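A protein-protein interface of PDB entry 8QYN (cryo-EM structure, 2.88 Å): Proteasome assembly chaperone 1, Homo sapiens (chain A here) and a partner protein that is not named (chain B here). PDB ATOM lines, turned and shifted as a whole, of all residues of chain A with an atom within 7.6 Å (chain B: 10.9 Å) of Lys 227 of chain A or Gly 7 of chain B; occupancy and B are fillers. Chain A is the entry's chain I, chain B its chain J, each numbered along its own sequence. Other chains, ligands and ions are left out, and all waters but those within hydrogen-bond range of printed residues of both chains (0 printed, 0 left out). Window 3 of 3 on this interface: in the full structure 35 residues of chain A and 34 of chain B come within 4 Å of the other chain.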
ATOM      1  N   PRO A 158      17.411 -39.529  -5.625  1.00  0.00           N
ATOM      2  CA  PRO A 158      16.631 -39.968  -6.788  1.00  0.00           C
ATOM      3  C   PRO A 158      17.414 -39.864  -8.087  1.00  0.00           C
ATOM      4  O   PRO A 158      18.603 -39.536  -8.079  1.00  0.00           O
ATOM      5  CB  PRO A 158      15.431 -39.014  -6.777  1.00  0.00           C
ATOM      6  CG  PRO A 158      15.966 -37.768  -6.158  1.00  0.00           C
ATOM      7  CD  PRO A 158      17.006 -38.192  -5.155  1.00  0.00           C
ATOM      8  N   ARG A 159      16.754 -40.144  -9.207  1.00  0.00           N
ATOM      9  CA  ARG A 159      17.373 -40.076 -10.521  1.00  0.00           C
ATOM     10  C   ARG A 159      16.791 -38.916 -11.317  1.00  0.00           C
ATOM     11  O   ARG A 159      15.624 -38.550 -11.155  1.00  0.00           O
ATOM     12  CB  ARG A 159      17.184 -41.385 -11.291  1.00  0.00           C
ATOM     13  CG  ARG A 159      18.279 -41.659 -12.308  1.00  0.00           C
ATOM     14  CD  ARG A 159      19.637 -41.781 -11.638  1.00  0.00           C
ATOM     15  NE  ARG A 159      19.691 -42.905 -10.710  1.00  0.00           N
ATOM     16  CZ  ARG A 159      19.945 -44.157 -11.065  1.00  0.00           C
ATOM     17  NH1 ARG A 159      20.169 -44.487 -12.326  1.00  0.00           N
ATOM     18  NH2 ARG A 159      19.974 -45.103 -10.130  1.00  0.00           N
ATOM     19  N   LYS A 160      17.626 -38.340 -12.183  1.00  0.00           N
ATOM     20  CA  LYS A 160      17.228 -37.144 -12.918  1.00  0.00           C
ATOM     21  C   LYS A 160      16.178 -37.461 -13.977  1.00  0.00           C
ATOM     22  O   LYS A 160      15.174 -36.751 -14.101  1.00  0.00           O
ATOM     23  CB  LYS A 160      18.457 -36.493 -13.554  1.00  0.00           C
ATOM     24  CG  LYS A 160      19.156 -35.482 -12.660  1.00  0.00           C
ATOM     25  CD  LYS A 160      19.997 -36.170 -11.597  1.00  0.00           C
ATOM     26  CE  LYS A 160      20.361 -35.212 -10.475  1.00  0.00           C
ATOM     27  NZ  LYS A 160      20.813 -35.937  -9.255  1.00  0.00           N
ATOM     28  N   ASN A 161      16.390 -38.522 -14.749  1.00  0.00           N
ATOM     29  CA  ASN A 161      15.533 -38.863 -15.882  1.00  0.00           C
ATOM     30  C   ASN A 161      14.649 -40.040 -15.488  1.00  0.00           C
ATOM     31  O   ASN A 161      15.083 -41.194 -15.530  1.00  0.00           O
ATOM     32  CB  ASN A 161      16.372 -39.189 -17.113  1.00  0.00           C
ATOM     33  CG  ASN A 161      17.383 -38.108 -17.430  1.00  0.00           C
ATOM     34  OD1 ASN A 161      18.589 -38.304 -17.271  1.00  0.00           O
ATOM     35  ND2 ASN A 161      16.899 -36.957 -17.883  1.00  0.00           N
ATOM     36  N   MET A 162      13.407 -39.744 -15.112  1.00  0.00           N
ATOM     37  CA  MET A 162      12.451 -40.776 -14.739  1.00  0.00           C
ATOM     38  C   MET A 162      11.059 -40.164 -14.723  1.00  0.00           C
ATOM     39  O   MET A 162      10.871 -39.056 -14.219  1.00  0.00           O
ATOM     40  CB  MET A 162      12.794 -41.382 -13.373  1.00  0.00           C
ATOM     41  CG  MET A 162      11.873 -42.506 -12.934  1.00  0.00           C
ATOM     42  SD  MET A 162      12.345 -43.198 -11.339  1.00  0.00           S
ATOM     43  CE  MET A 162      11.873 -41.872 -10.237  1.00  0.00           C
ATOM     44  N   THR A 194       2.600 -32.350 -11.752  1.00  0.00           N
ATOM     45  CA  THR A 194       3.592 -31.475 -11.151  1.00  0.00           C
ATOM     46  C   THR A 194       4.033 -30.404 -12.142  1.00  0.00           C
ATOM     47  O   THR A 194       3.637 -30.390 -13.309  1.00  0.00           O
ATOM     48  CB  THR A 194       4.801 -32.274 -10.671  1.00  0.00           C
ATOM     49  OG1 THR A 194       5.650 -32.572 -11.784  1.00  0.00           O
ATOM     50  CG2 THR A 194       4.359 -33.566 -10.015  1.00  0.00           C
ATOM     51  N   GLN A 195       4.871 -29.489 -11.653  1.00  0.00           N
ATOM     52  CA  GLN A 195       5.302 -28.361 -12.471  1.00  0.00           C
ATOM     53  C   GLN A 195       6.167 -28.815 -13.640  1.00  0.00           C
ATOM     54  O   GLN A 195       6.066 -28.264 -14.742  1.00  0.00           O
ATOM     55  CB  GLN A 195       6.054 -27.352 -11.603  1.00  0.00           C
ATOM     56  CG  GLN A 195       6.795 -26.284 -12.382  1.00  0.00           C
ATOM     57  CD  GLN A 195       8.298 -26.436 -12.286  1.00  0.00           C
ATOM     58  OE1 GLN A 195       8.832 -26.780 -11.233  1.00  0.00           O
ATOM     59  NE2 GLN A 195       8.989 -26.179 -13.389  1.00  0.00           N
ATOM     60  N   ASN A 196       7.008 -29.820 -13.425  1.00  0.00           N
ATOM     61  CA  ASN A 196       7.983 -30.244 -14.420  1.00  0.00           C
ATOM     62  C   ASN A 196       7.406 -31.201 -15.458  1.00  0.00           C
ATOM     63  O   ASN A 196       8.134 -31.612 -16.367  1.00  0.00           O
ATOM     64  CB  ASN A 196       9.180 -30.893 -13.723  1.00  0.00           C
ATOM     65  CG  ASN A 196      10.487 -30.581 -14.412  1.00  0.00           C
ATOM     66  OD1 ASN A 196      10.507 -29.961 -15.473  1.00  0.00           O
ATOM     67  ND2 ASN A 196      11.591 -30.996 -13.804  1.00  0.00           N
ATOM     68  N   SER A 221       3.939 -35.612  -3.628  1.00  0.00           N
ATOM     69  CA  SER A 221       4.725 -34.678  -2.833  1.00  0.00           C
ATOM     70  C   SER A 221       6.214 -34.953  -2.989  1.00  0.00           C
ATOM     71  O   SER A 221       7.010 -34.021  -3.160  1.00  0.00           O
ATOM     72  CB  SER A 221       4.311 -34.760  -1.367  1.00  0.00           C
ATOM     73  OG  SER A 221       2.906 -34.673  -1.236  1.00  0.00           O
ATOM     74  N   TYR A 222       6.603 -36.229  -2.954  1.00  0.00           N
ATOM     75  CA  TYR A 222       8.003 -36.582  -3.167  1.00  0.00           C
ATOM     76  C   TYR A 222       8.488 -36.102  -4.529  1.00  0.00           C
ATOM     77  O   TYR A 222       9.540 -35.457  -4.642  1.00  0.00           O
ATOM     78  CB  TYR A 222       8.176 -38.094  -3.031  1.00  0.00           C
ATOM     79  CG  TYR A 222       9.604 -38.574  -3.128  1.00  0.00           C
ATOM     80  CD1 TYR A 222      10.398 -38.681  -1.998  1.00  0.00           C
ATOM     81  CD2 TYR A 222      10.154 -38.931  -4.350  1.00  0.00           C
ATOM     82  CE1 TYR A 222      11.700 -39.122  -2.082  1.00  0.00           C
ATOM     83  CE2 TYR A 222      11.454 -39.371  -4.444  1.00  0.00           C
ATOM     84  CZ  TYR A 222      12.222 -39.464  -3.307  1.00  0.00           C
ATOM     85  OH  TYR A 222      13.521 -39.902  -3.394  1.00  0.00           O
ATOM     86  N   CYS A 223       7.713 -36.389  -5.579  1.00  0.00           N
ATOM     87  CA  CYS A 223       8.131 -36.030  -6.931  1.00  0.00           C
ATOM     88  C   CYS A 223       8.208 -34.519  -7.111  1.00  0.00           C
ATOM     89  O   CYS A 223       9.104 -34.016  -7.795  1.00  0.00           O
ATOM     90  CB  CYS A 223       7.179 -36.644  -7.954  1.00  0.00           C
ATOM     91  SG  CYS A 223       7.202 -38.447  -8.006  1.00  0.00           S
ATOM     92  N   GLN A 224       7.270 -33.780  -6.517  1.00  0.00           N
ATOM     93  CA  GLN A 224       7.273 -32.328  -6.653  1.00  0.00           C
ATOM     94  C   GLN A 224       8.442 -31.705  -5.905  1.00  0.00           C
ATOM     95  O   GLN A 224       9.093 -30.788  -6.417  1.00  0.00           O
ATOM     96  CB  GLN A 224       5.949 -31.752  -6.153  1.00  0.00           C
ATOM     97  CG  GLN A 224       5.976 -30.260  -5.875  1.00  0.00           C
ATOM     98  CD  GLN A 224       5.713 -29.428  -7.113  1.00  0.00           C
ATOM     99  OE1 GLN A 224       5.732 -29.933  -8.231  1.00  0.00           O
ATOM    100  NE2 GLN A 224       5.461 -28.142  -6.916  1.00  0.00           N
ATOM    101  N   VAL A 225       8.726 -32.187  -4.694  1.00  0.00           N
ATOM    102  CA  VAL A 225       9.839 -31.633  -3.929  1.00  0.00           C
ATOM    103  C   VAL A 225      11.162 -31.919  -4.626  1.00  0.00           C
ATOM    104  O   VAL A 225      12.034 -31.045  -4.715  1.00  0.00           O
ATOM    105  CB  VAL A 225       9.828 -32.177  -2.490  1.00  0.00           C
ATOM    106  CG1 VAL A 225      11.087 -31.758  -1.760  1.00  0.00           C
ATOM    107  CG2 VAL A 225       8.604 -31.681  -1.750  1.00  0.00           C
ATOM    108  N   TRP A 226      11.336 -33.135  -5.143  1.00  0.00           N
ATOM    109  CA  TRP A 226      12.622 -33.542  -5.698  1.00  0.00           C
ATOM    110  C   TRP A 226      12.722 -33.348  -7.208  1.00  0.00           C
ATOM    111  O   TRP A 226      13.665 -33.857  -7.821  1.00  0.00           O
ATOM    112  CB  TRP A 226      12.910 -34.998  -5.336  1.00  0.00           C
ATOM    113  CG  TRP A 226      13.187 -35.198  -3.879  1.00  0.00           C
ATOM    114  CD1 TRP A 226      12.548 -36.056  -3.041  1.00  0.00           C
ATOM    115  CD2 TRP A 226      14.169 -34.519  -3.086  1.00  0.00           C
ATOM    116  NE1 TRP A 226      13.070 -35.961  -1.776  1.00  0.00           N
ATOM    117  CE2 TRP A 226      14.067 -35.024  -1.777  1.00  0.00           C
ATOM    118  CE3 TRP A 226      15.126 -33.537  -3.356  1.00  0.00           C
ATOM    119  CZ2 TRP A 226      14.882 -34.580  -0.742  1.00  0.00           C
ATOM    120  CZ3 TRP A 226      15.933 -33.096  -2.326  1.00  0.00           C
ATOM    121  CH2 TRP A 226      15.807 -33.618  -1.036  1.00  0.00           C
ATOM    122  N   LYS A 227      11.779 -32.627  -7.816  1.00  0.00           N
ATOM    123  CA  LYS A 227      11.837 -32.254  -9.231  1.00  0.00           C
ATOM    124  C   LYS A 227      11.867 -33.486 -10.139  1.00  0.00           C
ATOM    125  O   LYS A 227      12.806 -33.706 -10.905  1.00  0.00           O
ATOM    126  CB  LYS A 227      13.037 -31.343  -9.506  1.00  0.00           C
ATOM    127  CG  LYS A 227      12.985 -30.021  -8.767  1.00  0.00           C
ATOM    128  CD  LYS A 227      14.160 -29.133  -9.133  1.00  0.00           C
ATOM    129  CE  LYS A 227      13.969 -27.728  -8.598  1.00  0.00           C
ATOM    130  NZ  LYS A 227      13.479 -27.741  -7.193  1.00  0.00           N
ATOM    131  N   ILE A 228      10.809 -34.283 -10.049  1.00  0.00           N
ATOM    132  CA  ILE A 228      10.619 -35.460 -10.888  1.00  0.00           C
ATOM    133  C   ILE A 228       9.281 -35.310 -11.598  1.00  0.00           C
ATOM    134  O   ILE A 228       8.279 -35.011 -10.945  1.00  0.00           O
ATOM    135  CB  ILE A 228      10.651 -36.771 -10.084  1.00  0.00           C
ATOM    136  CG1 ILE A 228      11.963 -36.896  -9.311  1.00  0.00           C
ATOM    137  CG2 ILE A 228      10.469 -37.960 -11.002  1.00  0.00           C
ATOM    138  CD1 ILE A 228      12.058 -38.153  -8.480  1.00  0.00           C
ATOM    139  N   PRO A 229       9.217 -35.478 -12.918  1.00  0.00           N
ATOM    140  CA  PRO A 229       7.918 -35.434 -13.601  1.00  0.00           C
ATOM    141  C   PRO A 229       6.989 -36.531 -13.100  1.00  0.00           C
ATOM    142  O   PRO A 229       7.416 -37.653 -12.826  1.00  0.00           O
ATOM    143  CB  PRO A 229       8.286 -35.637 -15.075  1.00  0.00           C
ATOM    144  CG  PRO A 229       9.714 -35.230 -15.169  1.00  0.00           C
ATOM    145  CD  PRO A 229      10.335 -35.612 -13.864  1.00  0.00           C
ATOM    146  N   ALA A 230       5.708 -36.196 -12.985  1.00  0.00           N
ATOM    147  CA  ALA A 230       4.717 -37.138 -12.485  1.00  0.00           C
ATOM    148  C   ALA A 230       3.329 -36.666 -12.885  1.00  0.00           C
ATOM    149  O   ALA A 230       3.133 -35.510 -13.264  1.00  0.00           O
ATOM    150  CB  ALA A 230       4.810 -37.296 -10.966  1.00  0.00           C
ATOM    151  N   MET B   2      14.001 -30.343   6.503  1.00  0.00           N
ATOM    152  CA  MET B   2      14.906 -29.363   5.918  1.00  0.00           C
ATOM    153  C   MET B   2      14.162 -28.447   4.958  1.00  0.00           C
ATOM    154  O   MET B   2      13.062 -28.763   4.517  1.00  0.00           O
ATOM    155  CB  MET B   2      16.057 -30.063   5.194  1.00  0.00           C
ATOM    156  CG  MET B   2      15.612 -30.988   4.075  1.00  0.00           C
ATOM    157  SD  MET B   2      16.993 -31.670   3.139  1.00  0.00           S
ATOM    158  CE  MET B   2      17.754 -30.178   2.507  1.00  0.00           C
ATOM    159  N   PHE B   3      14.770 -27.308   4.641  1.00  0.00           N
ATOM    160  CA  PHE B   3      14.191 -26.347   3.711  1.00  0.00           C
ATOM    161  C   PHE B   3      14.729 -26.639   2.316  1.00  0.00           C
ATOM    162  O   PHE B   3      15.930 -26.497   2.063  1.00  0.00           O
ATOM    163  CB  PHE B   3      14.516 -24.920   4.140  1.00  0.00           C
ATOM    164  CG  PHE B   3      14.070 -23.878   3.160  1.00  0.00           C
ATOM    165  CD1 PHE B   3      12.742 -23.516   3.074  1.00  0.00           C
ATOM    166  CD2 PHE B   3      14.981 -23.259   2.327  1.00  0.00           C
ATOM    167  CE1 PHE B   3      12.332 -22.559   2.174  1.00  0.00           C
ATOM    168  CE2 PHE B   3      14.574 -22.301   1.424  1.00  0.00           C
ATOM    169  CZ  PHE B   3      13.249 -21.951   1.349  1.00  0.00           C
ATOM    170  N   VAL B   4      13.846 -27.046   1.414  1.00  0.00           N
ATOM    171  CA  VAL B   4      14.203 -27.366   0.036  1.00  0.00           C
ATOM    172  C   VAL B   4      13.799 -26.186  -0.839  1.00  0.00           C
ATOM    173  O   VAL B   4      12.598 -25.899  -0.951  1.00  0.00           O
ATOM    174  CB  VAL B   4      13.524 -28.658  -0.438  1.00  0.00           C
ATOM    175  CG1 VAL B   4      13.968 -29.000  -1.842  1.00  0.00           C
ATOM    176  CG2 VAL B   4      13.840 -29.794   0.511  1.00  0.00           C
ATOM    177  N   PRO B   5      14.743 -25.483  -1.462  1.00  0.00           N
ATOM    178  CA  PRO B   5      14.376 -24.315  -2.269  1.00  0.00           C
ATOM    179  C   PRO B   5      13.538 -24.704  -3.474  1.00  0.00           C
ATOM    180  O   PRO B   5      13.674 -25.796  -4.029  1.00  0.00           O
ATOM    181  CB  PRO B   5      15.731 -23.738  -2.695  1.00  0.00           C
ATOM    182  CG  PRO B   5      16.667 -24.889  -2.617  1.00  0.00           C
ATOM    183  CD  PRO B   5      16.192 -25.730  -1.473  1.00  0.00           C
ATOM    184  N   CYS B   6      12.655 -23.790  -3.874  1.00  0.00           N
ATOM    185  CA  CYS B   6      11.809 -24.005  -5.039  1.00  0.00           C
ATOM    186  C   CYS B   6      12.540 -23.758  -6.350  1.00  0.00           C
ATOM    187  O   CYS B   6      12.037 -24.158  -7.404  1.00  0.00           O
ATOM    188  CB  CYS B   6      10.575 -23.103  -4.964  1.00  0.00           C
ATOM    189  SG  CYS B   6       9.170 -23.660  -5.947  1.00  0.00           S
ATOM    190  N   GLY B   7      13.704 -23.115  -6.310  1.00  0.00           N
ATOM    191  CA  GLY B   7      14.472 -22.856  -7.510  1.00  0.00           C
ATOM    192  C   GLY B   7      15.813 -23.557  -7.516  1.00  0.00           C
ATOM    193  O   GLY B   7      15.877 -24.786  -7.605  1.00  0.00           O
ATOM    194  N   GLU B   8      16.894 -22.786  -7.420  1.00  0.00           N
ATOM    195  CA  GLU B   8      18.248 -23.323  -7.435  1.00  0.00           C
ATOM    196  C   GLU B   8      18.978 -23.127  -6.116  1.00  0.00           C
ATOM    197  O   GLU B   8      19.483 -24.094  -5.540  1.00  0.00           O
ATOM    198  CB  GLU B   8      19.052 -22.682  -8.574  1.00  0.00           C
ATOM    199  CG  GLU B   8      18.858 -23.354  -9.920  1.00  0.00           C
ATOM    200  CD  GLU B   8      19.071 -22.404 -11.079  1.00  0.00           C
ATOM    201  OE1 GLU B   8      18.851 -21.187 -10.900  1.00  0.00           O
ATOM    202  OE2 GLU B   8      19.459 -22.872 -12.170  1.00  0.00           O
ATOM    203  N   SER B   9      19.052 -21.894  -5.621  1.00  0.00           N
ATOM    204  CA  SER B   9      19.712 -21.594  -4.360  1.00  0.00           C
ATOM    205  C   SER B   9      18.748 -20.857  -3.447  1.00  0.00           C
ATOM    206  O   SER B   9      18.033 -19.952  -3.887  1.00  0.00           O
ATOM    207  CB  SER B   9      20.976 -20.754  -4.574  1.00  0.00           C
ATOM    208  OG  SER B   9      20.650 -19.442  -4.999  1.00  0.00           O
ATOM    209  N   ALA B  10      18.735 -21.245  -2.175  1.00  0.00           N
ATOM    210  CA  ALA B  10      17.842 -20.621  -1.216  1.00  0.00           C
ATOM    211  C   ALA B  10      18.257 -19.172  -0.966  1.00  0.00           C
ATOM    212  O   ALA B  10      19.445 -18.844  -0.987  1.00  0.00           O
ATOM    213  CB  ALA B  10      17.841 -21.394   0.099  1.00  0.00           C
ATOM    214  N   PRO B  11      17.294 -18.284  -0.730  1.00  0.00           N
ATOM    215  CA  PRO B  11      17.639 -16.887  -0.438  1.00  0.00           C
ATOM    216  C   PRO B  11      18.188 -16.723   0.968  1.00  0.00           C
ATOM    217  O   PRO B  11      18.366 -17.707   1.691  1.00  0.00           O
ATOM    218  CB  PRO B  11      16.304 -16.146  -0.610  1.00  0.00           C
ATOM    219  CG  PRO B  11      15.347 -17.148  -1.200  1.00  0.00           C
ATOM    220  CD  PRO B  11      15.840 -18.488  -0.786  1.00  0.00           C
ATOM    221  N   SER B  43       4.952 -14.453  -2.384  1.00  0.00           N
ATOM    222  CA  SER B  43       5.310 -15.414  -3.416  1.00  0.00           C
ATOM    223  C   SER B  43       6.076 -16.584  -2.812  1.00  0.00           C
ATOM    224  O   SER B  43       6.879 -16.403  -1.892  1.00  0.00           O
ATOM    225  CB  SER B  43       6.151 -14.752  -4.508  1.00  0.00           C
ATOM    226  OG  SER B  43       5.601 -13.501  -4.880  1.00  0.00           O
ATOM    227  N   LYS B  44       5.826 -17.779  -3.340  1.00  0.00           N
ATOM    228  CA  LYS B  44       6.469 -18.982  -2.831  1.00  0.00           C
ATOM    229  C   LYS B  44       7.961 -18.973  -3.141  1.00  0.00           C
ATOM    230  O   LYS B  44       8.390 -18.487  -4.190  1.00  0.00           O
ATOM    231  CB  LYS B  44       5.816 -20.221  -3.438  1.00  0.00           C
ATOM    232  CG  LYS B  44       5.912 -21.462  -2.575  1.00  0.00           C
ATOM    233  CD  LYS B  44       4.901 -22.508  -3.003  1.00  0.00           C
ATOM    234  CE  LYS B  44       5.296 -23.144  -4.321  1.00  0.00           C
ATOM    235  NZ  LYS B  44       4.312 -24.169  -4.754  1.00  0.00           N
ATOM    236  N   ILE B  45       8.757 -19.517  -2.220  1.00  0.00           N
ATOM    237  CA  ILE B  45      10.205 -19.555  -2.395  1.00  0.00           C
ATOM    238  C   ILE B  45      10.746 -20.962  -2.181  1.00  0.00           C
ATOM    239  O   ILE B  45      11.877 -21.264  -2.576  1.00  0.00           O
ATOM    240  CB  ILE B  45      10.911 -18.562  -1.454  1.00  0.00           C
ATOM    241  CG1 ILE B  45      10.517 -18.825  -0.002  1.00  0.00           C
ATOM    242  CG2 ILE B  45      10.599 -17.135  -1.859  1.00  0.00           C
ATOM    243  CD1 ILE B  45      11.497 -18.270   1.003  1.00  0.00           C
ATOM    244  N   GLY B  46       9.962 -21.830  -1.555  1.00  0.00           N
ATOM    245  CA  GLY B  46      10.433 -23.181  -1.315  1.00  0.00           C
ATOM    246  C   GLY B  46       9.438 -23.972  -0.500  1.00  0.00           C
ATOM    247  O   GLY B  46       8.336 -23.508  -0.193  1.00  0.00           O
ATOM    248  N   TYR B  47       9.849 -25.189  -0.156  1.00  0.00           N
ATOM    249  CA  TYR B  47       9.051 -26.116   0.630  1.00  0.00           C
ATOM    250  C   TYR B  47       9.767 -26.440   1.934  1.00  0.00           C
ATOM    251  O   TYR B  47      10.906 -26.033   2.166  1.00  0.00           O
ATOM    252  CB  TYR B  47       8.773 -27.411  -0.145  1.00  0.00           C
ATOM    253  CG  TYR B  47       8.397 -27.199  -1.590  1.00  0.00           C
ATOM    254  CD1 TYR B  47       7.076 -26.998  -1.958  1.00  0.00           C
ATOM    255  CD2 TYR B  47       9.361 -27.204  -2.584  1.00  0.00           C
ATOM    256  CE1 TYR B  47       6.728 -26.804  -3.274  1.00  0.00           C
ATOM    257  CE2 TYR B  47       9.021 -27.010  -3.903  1.00  0.00           C
ATOM    258  CZ  TYR B  47       7.704 -26.810  -4.241  1.00  0.00           C
ATOM    259  OH  TYR B  47       7.361 -26.616  -5.557  1.00  0.00           O
ATOM    260  N   TYR B  49      10.108 -30.010   3.649  1.00  0.00           N
ATOM    261  CA  TYR B  49       9.819 -31.435   3.576  1.00  0.00           C
ATOM    262  C   TYR B  49      10.207 -32.109   4.887  1.00  0.00           C
ATOM    263  O   TYR B  49      11.363 -32.030   5.313  1.00  0.00           O
ATOM    264  CB  TYR B  49      10.554 -32.085   2.407  1.00  0.00           C
ATOM    265  CG  TYR B  49       9.954 -33.407   1.998  1.00  0.00           C
ATOM    266  CD1 TYR B  49       8.598 -33.518   1.732  1.00  0.00           C
ATOM    267  CD2 TYR B  49      10.737 -34.545   1.892  1.00  0.00           C
ATOM    268  CE1 TYR B  49       8.040 -34.720   1.367  1.00  0.00           C
ATOM    269  CE2 TYR B  49      10.186 -35.755   1.527  1.00  0.00           C
ATOM    270  CZ  TYR B  49       8.835 -35.836   1.266  1.00  0.00           C
ATOM    271  OH  TYR B  49       8.278 -37.036   0.901  1.00  0.00           O
ATOM    272  N   LEU B  72       0.749 -27.019  -8.415  1.00  0.00           N
ATOM    273  CA  LEU B  72       0.653 -28.002  -7.349  1.00  0.00           C
ATOM    274  C   LEU B  72       1.117 -27.417  -6.022  1.00  0.00           C
ATOM    275  O   LEU B  72       1.985 -26.544  -5.969  1.00  0.00           O
ATOM    276  CB  LEU B  72       1.478 -29.241  -7.682  1.00  0.00           C
ATOM    277  CG  LEU B  72       0.896 -30.539  -7.130  1.00  0.00           C
ATOM    278  CD1 LEU B  72      -0.416 -30.843  -7.820  1.00  0.00           C
ATOM    279  CD2 LEU B  72       1.872 -31.683  -7.295  1.00  0.00           C
ATOM    280  N   ILE B  74       1.770 -28.638  -1.654  1.00  0.00           N
ATOM    281  CA  ILE B  74       1.918 -29.731  -0.700  1.00  0.00           C
ATOM    282  C   ILE B  74       1.549 -29.225   0.688  1.00  0.00           C
ATOM    283  O   ILE B  74       1.132 -28.073   0.847  1.00  0.00           O
ATOM    284  CB  ILE B  74       3.340 -30.318  -0.733  1.00  0.00           C
ATOM    285  CG1 ILE B  74       4.349 -29.335  -0.145  1.00  0.00           C
ATOM    286  CG2 ILE B  74       3.729 -30.683  -2.154  1.00  0.00           C
ATOM    287  CD1 ILE B  74       5.667 -29.972   0.213  1.00  0.00           C
ATOM    288  N   VAL B  78       6.610 -22.358   2.068  1.00  0.00           N
ATOM    289  CA  VAL B  78       7.224 -21.168   2.647  1.00  0.00           C
ATOM    290  C   VAL B  78       7.096 -20.017   1.658  1.00  0.00           C
ATOM    291  O   VAL B  78       7.501 -20.142   0.498  1.00  0.00           O
ATOM    292  CB  VAL B  78       8.699 -21.415   3.006  1.00  0.00           C
ATOM    293  CG1 VAL B  78       9.364 -20.123   3.434  1.00  0.00           C
ATOM    294  CG2 VAL B  78       8.808 -22.458   4.096  1.00  0.00           C
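The side-chain hydroxyl (OH) of Tyr 47 of chain B lies within hydrogen-bond range of the side-chain amide nitrogen (NE2) of Gln 224 of chain A, 2.8 Å away.
The backbone carbonyl oxygen of Met 2 of chain B lies within hydrogen-bond range of the backbone NH of Tyr 49 of chain B, at 3.3 Å.
The backbone NH (N) of Tyr 47 of chain B lies within hydrogen-bond range of the backbone carbonyl oxygen (O) of Val 4 of chain B, at 2.9 Å.
The backbone NH of Cys 6 of chain B lies within hydrogen-bond range of the backbone carbonyl oxygen of Ile 45 of chain B (2.9 Å).
OH of Tyr 47 of chain B is in hydrogen-bond range of SG of Cys 6 of chain B, 3.5 Å away.
Tyr 222 of chain A touches Tyr 49 of chain B.
Leu 72 of chain B touches Gln 224 of chain A (O to NE2, 3.9 Å).
Val 4 of chain B touches Val 225 of chain A (CG1 to CG1, 3.99 Å).
CG2 of Val 225 of chain A touches CD1 of Tyr 49 of chain B (3.9 Å).
Val 225 of chain A touches Ile 74 of chain B.
O of Pro 5 of chain B touches NZ of Lys 227 of chain A (3.7 Å).
NZ of Lys 227 of chain A touches O of Cys 6 of chain B, at 3.9 Å.
Gly 7 of chain B touches Lys 227 of chain A.
Printed residues of chain B within 4 Å of Gln 224 of chain A: Tyr 47 (2.8 Å) and Leu 72 (3.9 Å).
Of chain B, only Pro 5 (3.7 Å), Cys 6 (3.9 Å) and Gly 7 (3.6 Å) come within 4 Å of Lys 227 of chain A.
Ile 228 of chain A touches none of the printed residues of chain B.
Pro 229 of chain A touches none of the printed residues of chain B.
Of the printed residues of chain A, Cys 6 of chain B touches Lys 227 (3.9 Å).
Of the printed residues of chain A, Leu 72 of chain B touches Gln 224.
The nearest residue of chain B that does not touch Lys 227 of chain A is Val 4 of chain B (5.5 Å).
The nearest printed residue of chain A that does not touch Gly 7 of chain B is Gln 195 of chain A (7.8 Å).
The nearest printed residue of chain B that does not touch Gln 224 of chain A is Ile 74 of chain B (4.4 Å).
Of the 18 printed residues of chain A, 4 touch a printed residue of chain B.
Along chain A the printed residues that touch a printed residue of chain B span positions 222 to 227.
Printed residues of chain B that touch a printed residue of chain A: Val 4, Pro 5, Cys 6, Gly 7, Tyr 47, Tyr 49, Leu 72 and Ile 74.
Among the printed residues, 9 pairs touch across the chains.
Among the printed residues, no Asp or Glu carboxylate lies within 4 Å of a Lys or Arg side-chain nitrogen of the other chain.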
